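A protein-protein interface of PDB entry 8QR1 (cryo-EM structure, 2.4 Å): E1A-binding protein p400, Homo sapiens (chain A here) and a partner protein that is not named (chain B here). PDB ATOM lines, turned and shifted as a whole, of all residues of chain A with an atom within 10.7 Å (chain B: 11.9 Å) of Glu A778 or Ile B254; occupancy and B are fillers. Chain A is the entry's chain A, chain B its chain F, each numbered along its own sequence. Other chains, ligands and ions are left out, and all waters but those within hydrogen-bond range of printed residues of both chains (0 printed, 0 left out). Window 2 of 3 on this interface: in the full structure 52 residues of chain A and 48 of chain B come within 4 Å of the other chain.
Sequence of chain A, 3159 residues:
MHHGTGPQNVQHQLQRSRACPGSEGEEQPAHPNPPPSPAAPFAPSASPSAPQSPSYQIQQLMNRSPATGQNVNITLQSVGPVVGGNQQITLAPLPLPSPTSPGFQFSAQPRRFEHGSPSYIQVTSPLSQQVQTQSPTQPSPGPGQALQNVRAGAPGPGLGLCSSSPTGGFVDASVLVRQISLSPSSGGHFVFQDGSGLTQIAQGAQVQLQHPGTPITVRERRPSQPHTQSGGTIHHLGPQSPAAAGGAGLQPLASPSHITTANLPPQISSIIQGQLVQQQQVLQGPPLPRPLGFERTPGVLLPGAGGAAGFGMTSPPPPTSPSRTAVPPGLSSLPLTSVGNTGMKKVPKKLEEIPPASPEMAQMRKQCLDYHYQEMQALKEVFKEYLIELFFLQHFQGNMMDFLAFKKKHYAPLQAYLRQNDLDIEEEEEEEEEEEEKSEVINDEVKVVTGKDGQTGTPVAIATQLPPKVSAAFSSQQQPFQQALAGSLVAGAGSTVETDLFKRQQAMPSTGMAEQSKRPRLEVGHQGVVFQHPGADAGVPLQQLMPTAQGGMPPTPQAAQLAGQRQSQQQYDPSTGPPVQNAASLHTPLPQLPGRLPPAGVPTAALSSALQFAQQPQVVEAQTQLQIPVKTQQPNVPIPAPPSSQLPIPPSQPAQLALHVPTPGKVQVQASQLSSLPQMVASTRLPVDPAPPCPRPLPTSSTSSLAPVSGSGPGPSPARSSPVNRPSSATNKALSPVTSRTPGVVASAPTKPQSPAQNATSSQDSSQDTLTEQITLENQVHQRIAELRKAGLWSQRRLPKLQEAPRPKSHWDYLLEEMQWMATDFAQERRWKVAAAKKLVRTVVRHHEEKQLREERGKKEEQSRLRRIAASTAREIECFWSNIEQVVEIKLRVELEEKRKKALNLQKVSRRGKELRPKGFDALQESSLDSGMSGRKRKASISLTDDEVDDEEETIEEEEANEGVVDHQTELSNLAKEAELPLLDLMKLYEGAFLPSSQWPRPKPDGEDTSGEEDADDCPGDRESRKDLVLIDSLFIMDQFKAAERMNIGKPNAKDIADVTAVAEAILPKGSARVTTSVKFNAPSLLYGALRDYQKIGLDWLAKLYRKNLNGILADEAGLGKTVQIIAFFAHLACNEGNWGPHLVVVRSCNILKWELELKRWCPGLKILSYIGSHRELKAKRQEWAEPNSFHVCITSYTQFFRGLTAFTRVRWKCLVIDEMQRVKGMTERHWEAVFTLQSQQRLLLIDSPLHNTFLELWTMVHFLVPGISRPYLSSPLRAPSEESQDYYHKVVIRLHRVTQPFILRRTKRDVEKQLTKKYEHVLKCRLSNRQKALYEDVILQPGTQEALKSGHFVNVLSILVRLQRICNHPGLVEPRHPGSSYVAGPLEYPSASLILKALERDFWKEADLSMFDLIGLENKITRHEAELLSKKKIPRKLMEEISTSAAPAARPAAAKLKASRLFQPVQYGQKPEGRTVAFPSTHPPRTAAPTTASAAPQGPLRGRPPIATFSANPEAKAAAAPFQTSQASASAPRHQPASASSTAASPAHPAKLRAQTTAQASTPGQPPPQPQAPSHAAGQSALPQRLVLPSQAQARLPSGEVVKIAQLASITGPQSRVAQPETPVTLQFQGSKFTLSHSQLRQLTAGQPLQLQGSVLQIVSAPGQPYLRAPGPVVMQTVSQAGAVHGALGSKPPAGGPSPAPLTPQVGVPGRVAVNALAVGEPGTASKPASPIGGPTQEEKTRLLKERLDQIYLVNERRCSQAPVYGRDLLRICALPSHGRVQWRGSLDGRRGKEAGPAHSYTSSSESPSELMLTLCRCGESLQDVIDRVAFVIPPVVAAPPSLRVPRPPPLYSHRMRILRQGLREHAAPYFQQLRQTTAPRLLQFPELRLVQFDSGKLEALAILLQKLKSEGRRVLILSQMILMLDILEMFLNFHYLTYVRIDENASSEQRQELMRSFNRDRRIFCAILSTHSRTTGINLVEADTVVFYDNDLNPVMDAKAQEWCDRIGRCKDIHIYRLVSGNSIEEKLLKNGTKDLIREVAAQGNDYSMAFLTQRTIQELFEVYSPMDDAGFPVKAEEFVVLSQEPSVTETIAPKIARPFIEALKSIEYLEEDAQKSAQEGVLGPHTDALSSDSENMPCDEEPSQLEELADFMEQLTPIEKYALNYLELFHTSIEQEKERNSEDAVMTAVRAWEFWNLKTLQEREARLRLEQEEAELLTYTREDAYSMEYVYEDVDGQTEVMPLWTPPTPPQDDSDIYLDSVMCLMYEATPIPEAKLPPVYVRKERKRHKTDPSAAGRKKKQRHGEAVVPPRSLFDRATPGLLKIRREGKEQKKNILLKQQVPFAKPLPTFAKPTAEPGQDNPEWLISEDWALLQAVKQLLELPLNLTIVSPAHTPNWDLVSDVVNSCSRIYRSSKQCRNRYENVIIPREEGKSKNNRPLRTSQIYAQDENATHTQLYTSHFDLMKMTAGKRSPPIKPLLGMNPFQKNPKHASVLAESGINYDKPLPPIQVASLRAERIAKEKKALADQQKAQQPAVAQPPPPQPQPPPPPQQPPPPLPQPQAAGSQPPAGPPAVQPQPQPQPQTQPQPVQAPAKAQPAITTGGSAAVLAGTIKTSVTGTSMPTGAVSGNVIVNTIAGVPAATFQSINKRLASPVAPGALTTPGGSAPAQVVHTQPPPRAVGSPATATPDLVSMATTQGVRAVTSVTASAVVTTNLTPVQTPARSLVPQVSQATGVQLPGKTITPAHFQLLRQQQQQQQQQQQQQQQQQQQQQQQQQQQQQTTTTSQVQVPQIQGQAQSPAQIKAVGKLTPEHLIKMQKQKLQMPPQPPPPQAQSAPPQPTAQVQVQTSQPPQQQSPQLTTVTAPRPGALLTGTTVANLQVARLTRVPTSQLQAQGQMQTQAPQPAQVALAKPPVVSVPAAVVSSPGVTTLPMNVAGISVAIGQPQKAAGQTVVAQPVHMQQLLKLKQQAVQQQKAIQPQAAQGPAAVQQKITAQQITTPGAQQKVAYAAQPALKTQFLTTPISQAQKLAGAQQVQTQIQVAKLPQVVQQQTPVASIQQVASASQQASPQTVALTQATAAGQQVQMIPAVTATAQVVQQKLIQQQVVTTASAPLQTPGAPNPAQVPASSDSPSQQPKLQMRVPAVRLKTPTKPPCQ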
ATOM      1  N   ILE A 775      14.292 -18.761   9.933  1.00  0.00           N
ATOM      2  CA  ILE A 775      13.682 -18.906   8.579  1.00  0.00           C
ATOM      3  C   ILE A 775      13.798 -17.596   7.790  1.00  0.00           C
ATOM      4  O   ILE A 775      13.905 -17.616   6.564  1.00  0.00           O
ATOM      5  CB  ILE A 775      12.192 -19.387   8.688  1.00  0.00           C
ATOM      6  CG1 ILE A 775      11.529 -19.582   7.312  1.00  0.00           C
ATOM      7  CG2 ILE A 775      11.345 -18.427   9.540  1.00  0.00           C
ATOM      8  CD1 ILE A 775      12.236 -20.558   6.385  1.00  0.00           C
ATOM      9  N   THR A 776      13.773 -16.461   8.495  1.00  0.00           N
ATOM     10  CA  THR A 776      13.793 -15.167   7.819  1.00  0.00           C
ATOM     11  C   THR A 776      15.123 -14.902   7.123  1.00  0.00           C
ATOM     12  O   THR A 776      15.165 -14.159   6.135  1.00  0.00           O
ATOM     13  CB  THR A 776      13.499 -14.050   8.822  1.00  0.00           C
ATOM     14  OG1 THR A 776      14.443 -14.107   9.898  1.00  0.00           O
ATOM     15  CG2 THR A 776      12.088 -14.188   9.380  1.00  0.00           C
ATOM     16  N   LEU A 777      16.216 -15.496   7.610  1.00  0.00           N
ATOM     17  CA  LEU A 777      17.539 -15.248   7.039  1.00  0.00           C
ATOM     18  C   LEU A 777      17.815 -16.056   5.770  1.00  0.00           C
ATOM     19  O   LEU A 777      18.916 -15.930   5.219  1.00  0.00           O
ATOM     20  CB  LEU A 777      18.627 -15.526   8.089  1.00  0.00           C
ATOM     21  CG  LEU A 777      18.651 -16.805   8.944  1.00  0.00           C
ATOM     22  CD1 LEU A 777      18.793 -18.081   8.123  1.00  0.00           C
ATOM     23  CD2 LEU A 777      19.784 -16.706   9.957  1.00  0.00           C
ATOM     24  N   GLU A 778      16.867 -16.874   5.302  1.00  0.00           N
ATOM     25  CA  GLU A 778      17.091 -17.674   4.101  1.00  0.00           C
ATOM     26  C   GLU A 778      17.319 -16.790   2.879  1.00  0.00           C
ATOM     27  O   GLU A 778      18.230 -17.045   2.077  1.00  0.00           O
ATOM     28  CB  GLU A 778      15.896 -18.608   3.890  1.00  0.00           C
ATOM     29  CG  GLU A 778      15.924 -19.430   2.600  1.00  0.00           C
ATOM     30  CD  GLU A 778      15.077 -18.842   1.478  1.00  0.00           C
ATOM     31  OE1 GLU A 778      14.760 -17.633   1.508  1.00  0.00           O
ATOM     32  OE2 GLU A 778      14.720 -19.604   0.554  1.00  0.00           O
ATOM     33  N   ASN A 779      16.509 -15.740   2.724  1.00  0.00           N
ATOM     34  CA  ASN A 779      16.726 -14.803   1.627  1.00  0.00           C
ATOM     35  C   ASN A 779      18.052 -14.071   1.778  1.00  0.00           C
ATOM     36  O   ASN A 779      18.709 -13.777   0.776  1.00  0.00           O
ATOM     37  CB  ASN A 779      15.565 -13.808   1.540  1.00  0.00           C
ATOM     38  CG  ASN A 779      15.401 -12.974   2.801  1.00  0.00           C
ATOM     39  OD1 ASN A 779      16.227 -12.113   3.106  1.00  0.00           O
ATOM     40  ND2 ASN A 779      14.327 -13.228   3.542  1.00  0.00           N
ATOM     41  N   GLN A 780      18.469 -13.784   3.014  1.00  0.00           N
ATOM     42  CA  GLN A 780      19.781 -13.183   3.230  1.00  0.00           C
ATOM     43  C   GLN A 780      20.895 -14.137   2.813  1.00  0.00           C
ATOM     44  O   GLN A 780      21.902 -13.710   2.234  1.00  0.00           O
ATOM     45  CB  GLN A 780      19.931 -12.783   4.699  1.00  0.00           C
ATOM     46  CG  GLN A 780      21.103 -11.835   4.995  1.00  0.00           C
ATOM     47  CD  GLN A 780      22.436 -12.543   5.227  1.00  0.00           C
ATOM     48  OE1 GLN A 780      22.485 -13.736   5.525  1.00  0.00           O
ATOM     49  NE2 GLN A 780      23.525 -11.797   5.087  1.00  0.00           N
ATOM     50  N   VAL A 781      20.732 -15.428   3.110  1.00  0.00           N
ATOM     51  CA  VAL A 781      21.737 -16.417   2.729  1.00  0.00           C
ATOM     52  C   VAL A 781      21.828 -16.515   1.211  1.00  0.00           C
ATOM     53  O   VAL A 781      22.920 -16.640   0.643  1.00  0.00           O
ATOM     54  CB  VAL A 781      21.420 -17.783   3.372  1.00  0.00           C
ATOM     55  CG1 VAL A 781      22.284 -18.889   2.781  1.00  0.00           C
ATOM     56  CG2 VAL A 781      21.630 -17.732   4.880  1.00  0.00           C
ATOM     57  N   HIS A 782      20.679 -16.472   0.532  1.00  0.00           N
ATOM     58  CA  HIS A 782      20.699 -16.456  -0.928  1.00  0.00           C
ATOM     59  C   HIS A 782      21.343 -15.180  -1.458  1.00  0.00           C
ATOM     60  O   HIS A 782      22.069 -15.211  -2.459  1.00  0.00           O
ATOM     61  CB  HIS A 782      19.282 -16.602  -1.479  1.00  0.00           C
ATOM     62  CG  HIS A 782      18.681 -17.956  -1.256  1.00  0.00           C
ATOM     63  ND1 HIS A 782      19.374 -19.126  -1.480  1.00  0.00           N
ATOM     64  CD2 HIS A 782      17.445 -18.324  -0.846  1.00  0.00           C
ATOM     65  CE1 HIS A 782      18.593 -20.156  -1.206  1.00  0.00           C
ATOM     66  NE2 HIS A 782      17.418 -19.697  -0.820  1.00  0.00           N
ATOM     67  N   GLN A 783      21.081 -14.045  -0.804  1.00  0.00           N
ATOM     68  CA  GLN A 783      21.610 -12.770  -1.276  1.00  0.00           C
ATOM     69  C   GLN A 783      23.127 -12.720  -1.158  1.00  0.00           C
ATOM     70  O   GLN A 783      23.811 -12.252  -2.075  1.00  0.00           O
ATOM     71  CB  GLN A 783      20.968 -11.627  -0.489  1.00  0.00           C
ATOM     72  CG  GLN A 783      21.491 -10.233  -0.833  1.00  0.00           C
ATOM     73  CD  GLN A 783      20.629  -9.124  -0.257  1.00  0.00           C
ATOM     74  OE1 GLN A 783      19.621  -9.380   0.401  1.00  0.00           O
ATOM     75  NE2 GLN A 783      21.027  -7.882  -0.503  1.00  0.00           N
ATOM     76  N   ARG A 784      23.671 -13.190  -0.034  1.00  0.00           N
ATOM     77  CA  ARG A 784      25.118 -13.141   0.147  1.00  0.00           C
ATOM     78  C   ARG A 784      25.824 -14.100  -0.803  1.00  0.00           C
ATOM     79  O   ARG A 784      26.932 -13.815  -1.270  1.00  0.00           O
ATOM     80  CB  ARG A 784      25.477 -13.449   1.604  1.00  0.00           C
ATOM     81  CG  ARG A 784      26.978 -13.416   1.951  1.00  0.00           C
ATOM     82  CD  ARG A 784      27.650 -12.084   1.644  1.00  0.00           C
ATOM     83  NE  ARG A 784      29.067 -12.107   1.991  1.00  0.00           N
ATOM     84  CZ  ARG A 784      30.002 -11.304   1.492  1.00  0.00           C
ATOM     85  NH1 ARG A 784      29.714 -10.340   0.628  1.00  0.00           N
ATOM     86  NH2 ARG A 784      31.265 -11.469   1.873  1.00  0.00           N
ATOM     87  N   ILE A 785      25.202 -15.243  -1.092  1.00  0.00           N
ATOM     88  CA  ILE A 785      25.782 -16.183  -2.048  1.00  0.00           C
ATOM     89  C   ILE A 785      25.809 -15.565  -3.440  1.00  0.00           C
ATOM     90  O   ILE A 785      26.733 -15.806  -4.225  1.00  0.00           O
ATOM     91  CB  ILE A 785      25.006 -17.516  -2.021  1.00  0.00           C
ATOM     92  CG1 ILE A 785      25.278 -18.256  -0.706  1.00  0.00           C
ATOM     93  CG2 ILE A 785      25.391 -18.399  -3.216  1.00  0.00           C
ATOM     94  CD1 ILE A 785      24.281 -19.343  -0.370  1.00  0.00           C
ATOM     95  N   ALA A 786      24.789 -14.770  -3.772  1.00  0.00           N
ATOM     96  CA  ALA A 786      24.773 -14.087  -5.059  1.00  0.00           C
ATOM     97  C   ALA A 786      25.904 -13.073  -5.158  1.00  0.00           C
ATOM     98  O   ALA A 786      26.488 -12.886  -6.231  1.00  0.00           O
ATOM     99  CB  ALA A 786      23.423 -13.405  -5.269  1.00  0.00           C
ATOM    100  N   GLU B 245      31.880 -21.672   3.972  1.00  0.00           N
ATOM    101  CA  GLU B 245      31.477 -22.921   4.613  1.00  0.00           C
ATOM    102  C   GLU B 245      30.162 -22.755   5.361  1.00  0.00           C
ATOM    103  O   GLU B 245      29.308 -23.647   5.331  1.00  0.00           O
ATOM    104  CB  GLU B 245      32.574 -23.415   5.569  1.00  0.00           C
ATOM    105  CG  GLU B 245      33.476 -24.601   5.125  1.00  0.00           C
ATOM    106  CD  GLU B 245      32.769 -25.797   4.471  1.00  0.00           C
ATOM    107  OE1 GLU B 245      33.484 -26.690   3.976  1.00  0.00           O
ATOM    108  OE2 GLU B 245      31.525 -25.898   4.510  1.00  0.00           O
ATOM    109  N   TYR B 246      29.984 -21.615   6.031  1.00  0.00           N
ATOM    110  CA  TYR B 246      28.749 -21.357   6.765  1.00  0.00           C
ATOM    111  C   TYR B 246      27.584 -21.301   5.782  1.00  0.00           C
ATOM    112  O   TYR B 246      26.525 -21.884   6.025  1.00  0.00           O
ATOM    113  CB  TYR B 246      28.910 -20.038   7.544  1.00  0.00           C
ATOM    114  CG  TYR B 246      27.719 -19.323   8.213  1.00  0.00           C
ATOM    115  CD1 TYR B 246      26.477 -19.933   8.456  1.00  0.00           C
ATOM    116  CD2 TYR B 246      27.850 -17.990   8.547  1.00  0.00           C
ATOM    117  CE1 TYR B 246      25.444 -19.234   9.050  1.00  0.00           C
ATOM    118  CE2 TYR B 246      26.820 -17.288   9.136  1.00  0.00           C
ATOM    119  CZ  TYR B 246      25.622 -17.904   9.382  1.00  0.00           C
ATOM    120  OH  TYR B 246      24.615 -17.172   9.969  1.00  0.00           O
ATOM    121  N   LEU B 247      27.764 -20.592   4.664  1.00  0.00           N
ATOM    122  CA  LEU B 247      26.675 -20.446   3.700  1.00  0.00           C
ATOM    123  C   LEU B 247      26.339 -21.777   3.034  1.00  0.00           C
ATOM    124  O   LEU B 247      25.160 -22.101   2.831  1.00  0.00           O
ATOM    125  CB  LEU B 247      27.046 -19.399   2.653  1.00  0.00           C
ATOM    126  CG  LEU B 247      27.191 -17.963   3.171  1.00  0.00           C
ATOM    127  CD1 LEU B 247      27.953 -17.100   2.179  1.00  0.00           C
ATOM    128  CD2 LEU B 247      25.840 -17.344   3.481  1.00  0.00           C
ATOM    129  N   LEU B 248      27.361 -22.565   2.691  1.00  0.00           N
ATOM    130  CA  LEU B 248      27.117 -23.881   2.110  1.00  0.00           C
ATOM    131  C   LEU B 248      26.424 -24.803   3.103  1.00  0.00           C
ATOM    132  O   LEU B 248      25.534 -25.572   2.725  1.00  0.00           O
ATOM    133  CB  LEU B 248      28.438 -24.488   1.634  1.00  0.00           C
ATOM    134  CG  LEU B 248      28.397 -25.643   0.628  1.00  0.00           C
ATOM    135  CD1 LEU B 248      27.759 -25.236  -0.692  1.00  0.00           C
ATOM    136  CD2 LEU B 248      29.805 -26.175   0.399  1.00  0.00           C
ATOM    137  N   GLN B 249      26.809 -24.735   4.379  1.00  0.00           N
ATOM    138  CA  GLN B 249      26.142 -25.536   5.397  1.00  0.00           C
ATOM    139  C   GLN B 249      24.693 -25.104   5.581  1.00  0.00           C
ATOM    140  O   GLN B 249      23.812 -25.942   5.800  1.00  0.00           O
ATOM    141  CB  GLN B 249      26.906 -25.428   6.714  1.00  0.00           C
ATOM    142  CG  GLN B 249      26.583 -26.535   7.727  1.00  0.00           C
ATOM    143  CD  GLN B 249      26.015 -26.045   9.058  1.00  0.00           C
ATOM    144  OE1 GLN B 249      25.534 -24.919   9.190  1.00  0.00           O
ATOM    145  NE2 GLN B 249      26.067 -26.915  10.058  1.00  0.00           N
ATOM    146  N   GLU B 250      24.431 -23.797   5.510  1.00  0.00           N
ATOM    147  CA  GLU B 250      23.058 -23.306   5.594  1.00  0.00           C
ATOM    148  C   GLU B 250      22.219 -23.815   4.433  1.00  0.00           C
ATOM    149  O   GLU B 250      21.069 -24.229   4.626  1.00  0.00           O
ATOM    150  CB  GLU B 250      23.047 -21.778   5.629  1.00  0.00           C
ATOM    151  CG  GLU B 250      23.493 -21.157   6.951  1.00  0.00           C
ATOM    152  CD  GLU B 250      22.500 -21.369   8.071  1.00  0.00           C
ATOM    153  OE1 GLU B 250      21.310 -21.044   7.879  1.00  0.00           O
ATOM    154  OE2 GLU B 250      22.913 -21.846   9.149  1.00  0.00           O
ATOM    155  N   LEU B 251      22.776 -23.792   3.221  1.00  0.00           N
ATOM    156  CA  LEU B 251      22.064 -24.350   2.072  1.00  0.00           C
ATOM    157  C   LEU B 251      21.820 -25.841   2.261  1.00  0.00           C
ATOM    158  O   LEU B 251      20.735 -26.351   1.957  1.00  0.00           O
ATOM    159  CB  LEU B 251      22.842 -24.105   0.774  1.00  0.00           C
ATOM    160  CG  LEU B 251      22.324 -23.023  -0.179  1.00  0.00           C
ATOM    161  CD1 LEU B 251      22.101 -21.700   0.535  1.00  0.00           C
ATOM    162  CD2 LEU B 251      23.288 -22.844  -1.343  1.00  0.00           C
ATOM    163  N   ARG B 252      22.824 -26.551   2.782  1.00  0.00           N
ATOM    164  CA  ARG B 252      22.709 -27.990   2.991  1.00  0.00           C
ATOM    165  C   ARG B 252      21.607 -28.315   3.990  1.00  0.00           C
ATOM    166  O   ARG B 252      20.818 -29.244   3.775  1.00  0.00           O
ATOM    167  CB  ARG B 252      24.054 -28.537   3.481  1.00  0.00           C
ATOM    168  CG  ARG B 252      24.197 -30.065   3.515  1.00  0.00           C
ATOM    169  CD  ARG B 252      24.085 -30.716   2.138  1.00  0.00           C
ATOM    170  NE  ARG B 252      25.041 -30.140   1.190  1.00  0.00           N
ATOM    171  CZ  ARG B 252      24.803 -29.788  -0.070  1.00  0.00           C
ATOM    172  NH1 ARG B 252      23.629 -29.986  -0.655  1.00  0.00           N
ATOM    173  NH2 ARG B 252      25.780 -29.224  -0.776  1.00  0.00           N
ATOM    174  N   LYS B 253      21.529 -27.553   5.082  1.00  0.00           N
ATOM    175  CA  LYS B 253      20.544 -27.846   6.116  1.00  0.00           C
ATOM    176  C   LYS B 253      19.145 -27.406   5.695  1.00  0.00           C
ATOM    177  O   LYS B 253      18.165 -28.094   6.004  1.00  0.00           O
ATOM    178  CB  LYS B 253      20.959 -27.194   7.444  1.00  0.00           C
ATOM    179  CG  LYS B 253      20.445 -25.777   7.712  1.00  0.00           C
ATOM    180  CD  LYS B 253      21.130 -25.158   8.916  1.00  0.00           C
ATOM    181  CE  LYS B 253      20.399 -23.909   9.385  1.00  0.00           C
ATOM    182  NZ  LYS B 253      21.156 -23.181  10.439  1.00  0.00           N
ATOM    183  N   ILE B 254      19.028 -26.283   4.981  1.00  0.00           N
ATOM    184  CA  ILE B 254      17.708 -25.756   4.650  1.00  0.00           C
ATOM    185  C   ILE B 254      17.104 -26.485   3.454  1.00  0.00           C
ATOM    186  O   ILE B 254      15.879 -26.625   3.370  1.00  0.00           O
ATOM    187  CB  ILE B 254      17.796 -24.233   4.418  1.00  0.00           C
ATOM    188  CG1 ILE B 254      16.423 -23.560   4.591  1.00  0.00           C
ATOM    189  CG2 ILE B 254      18.407 -23.913   3.055  1.00  0.00           C
ATOM    190  CD1 ILE B 254      16.513 -22.068   4.832  1.00  0.00           C
ATOM    191  N   GLU B 255      17.932 -26.965   2.521  1.00  0.00           N
ATOM    192  CA  GLU B 255      17.429 -27.754   1.404  1.00  0.00           C
ATOM    193  C   GLU B 255      17.120 -29.197   1.785  1.00  0.00           C
ATOM    194  O   GLU B 255      16.494 -29.904   0.987  1.00  0.00           O
ATOM    195  CB  GLU B 255      18.439 -27.737   0.252  1.00  0.00           C
ATOM    196  CG  GLU B 255      18.591 -26.378  -0.428  1.00  0.00           C
ATOM    197  CD  GLU B 255      17.382 -25.981  -1.262  1.00  0.00           C
ATOM    198  OE1 GLU B 255      16.449 -26.801  -1.403  1.00  0.00           O
ATOM    199  OE2 GLU B 255      17.365 -24.844  -1.776  1.00  0.00           O
ATOM    200  N   ALA B 256      17.539 -29.652   2.964  1.00  0.00           N
ATOM    201  CA  ALA B 256      17.246 -31.006   3.420  1.00  0.00           C
ATOM    202  C   ALA B 256      17.224 -31.060   4.944  1.00  0.00           C
ATOM    203  O   ALA B 256      16.726 -32.018   5.534  1.00  0.00           O
ATOM    204  CB  ALA B 256      18.270 -31.982   2.869  1.00  0.00           C
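Printed residues of chain B within 4 Å of Glu A778: Ile B254 (3.5 Å). Of the printed residues of chain A, Ile B254 touches Glu A778 (3.5 Å). No residue of chain B comes within 4 Å of Asn A779. Of chain B, only Leu B247 (3.9 Å) and Leu B251 (3.6 Å) come within 4 Å of Val A781. No residue of chain B comes within 4 Å of His A782. No residue of chain A comes within 4 Å of Glu B255. No residue of chain A comes within 4 Å of Ala B256. Printed residues of chain B within 4 Å of Arg A784: Leu B247 (3.8 Å). Of the printed residues of chain A, Glu B250 touches Leu A777 (3.9 Å). Printed residues of chain A within 4 Å of Leu B247: Val A781, Arg A784 and Ile A785. Leu B248 touches none of the printed residues of chain A. The nearest residue of chain B that does not touch Glu A778 is Leu B251 (6.2 Å). The nearest residue of chain A that does not touch Ile B254 is Ile A775 (4.8 Å). The nearest printed residue of chain B that does not touch Ile A785 is Leu B248 (5.4 Å).
OE1 of Glu B250 touches CD1 of Leu A777, 3.9 Å away. Glu A778 touches Ile B254 (CG to CD1, 3.5 Å). Val A781 touches Leu B247. Leu B251 touches Val A781. CD1 of Leu B247 touches CG of Arg A784, at 3.8 Å. Ile A785 touches Leu B247 (CG1 to CB, 3.96 Å). Leu B251 touches Ile A785.
The side-chain carboxylate (OE2) of Glu A778 sits at hydrogen-bond distance from a ring nitrogen (NE2) of His A782 (3.0 Å). OE2 of Glu B250 is in salt-bridge range of NZ of Lys B253, at 2.6 Å.
Of the 12 printed residues of chain A, 5 touch a printed residue of chain B. Printed residues of chain A that touch a printed residue of chain B: Leu A777, Glu A778, Val A781, Arg A784 and Ile A785. Hydrophobic or aromatic side chains of chain A within 4 Å of the printed part of chain B: Leu A777, Val A781 and Ile A785. Among the printed residues, 7 pairs touch across the chains. Among the printed residues, no Asp or Glu carboxylate lies within 4 Å of a Lys or Arg side-chain nitrogen of the other chain.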
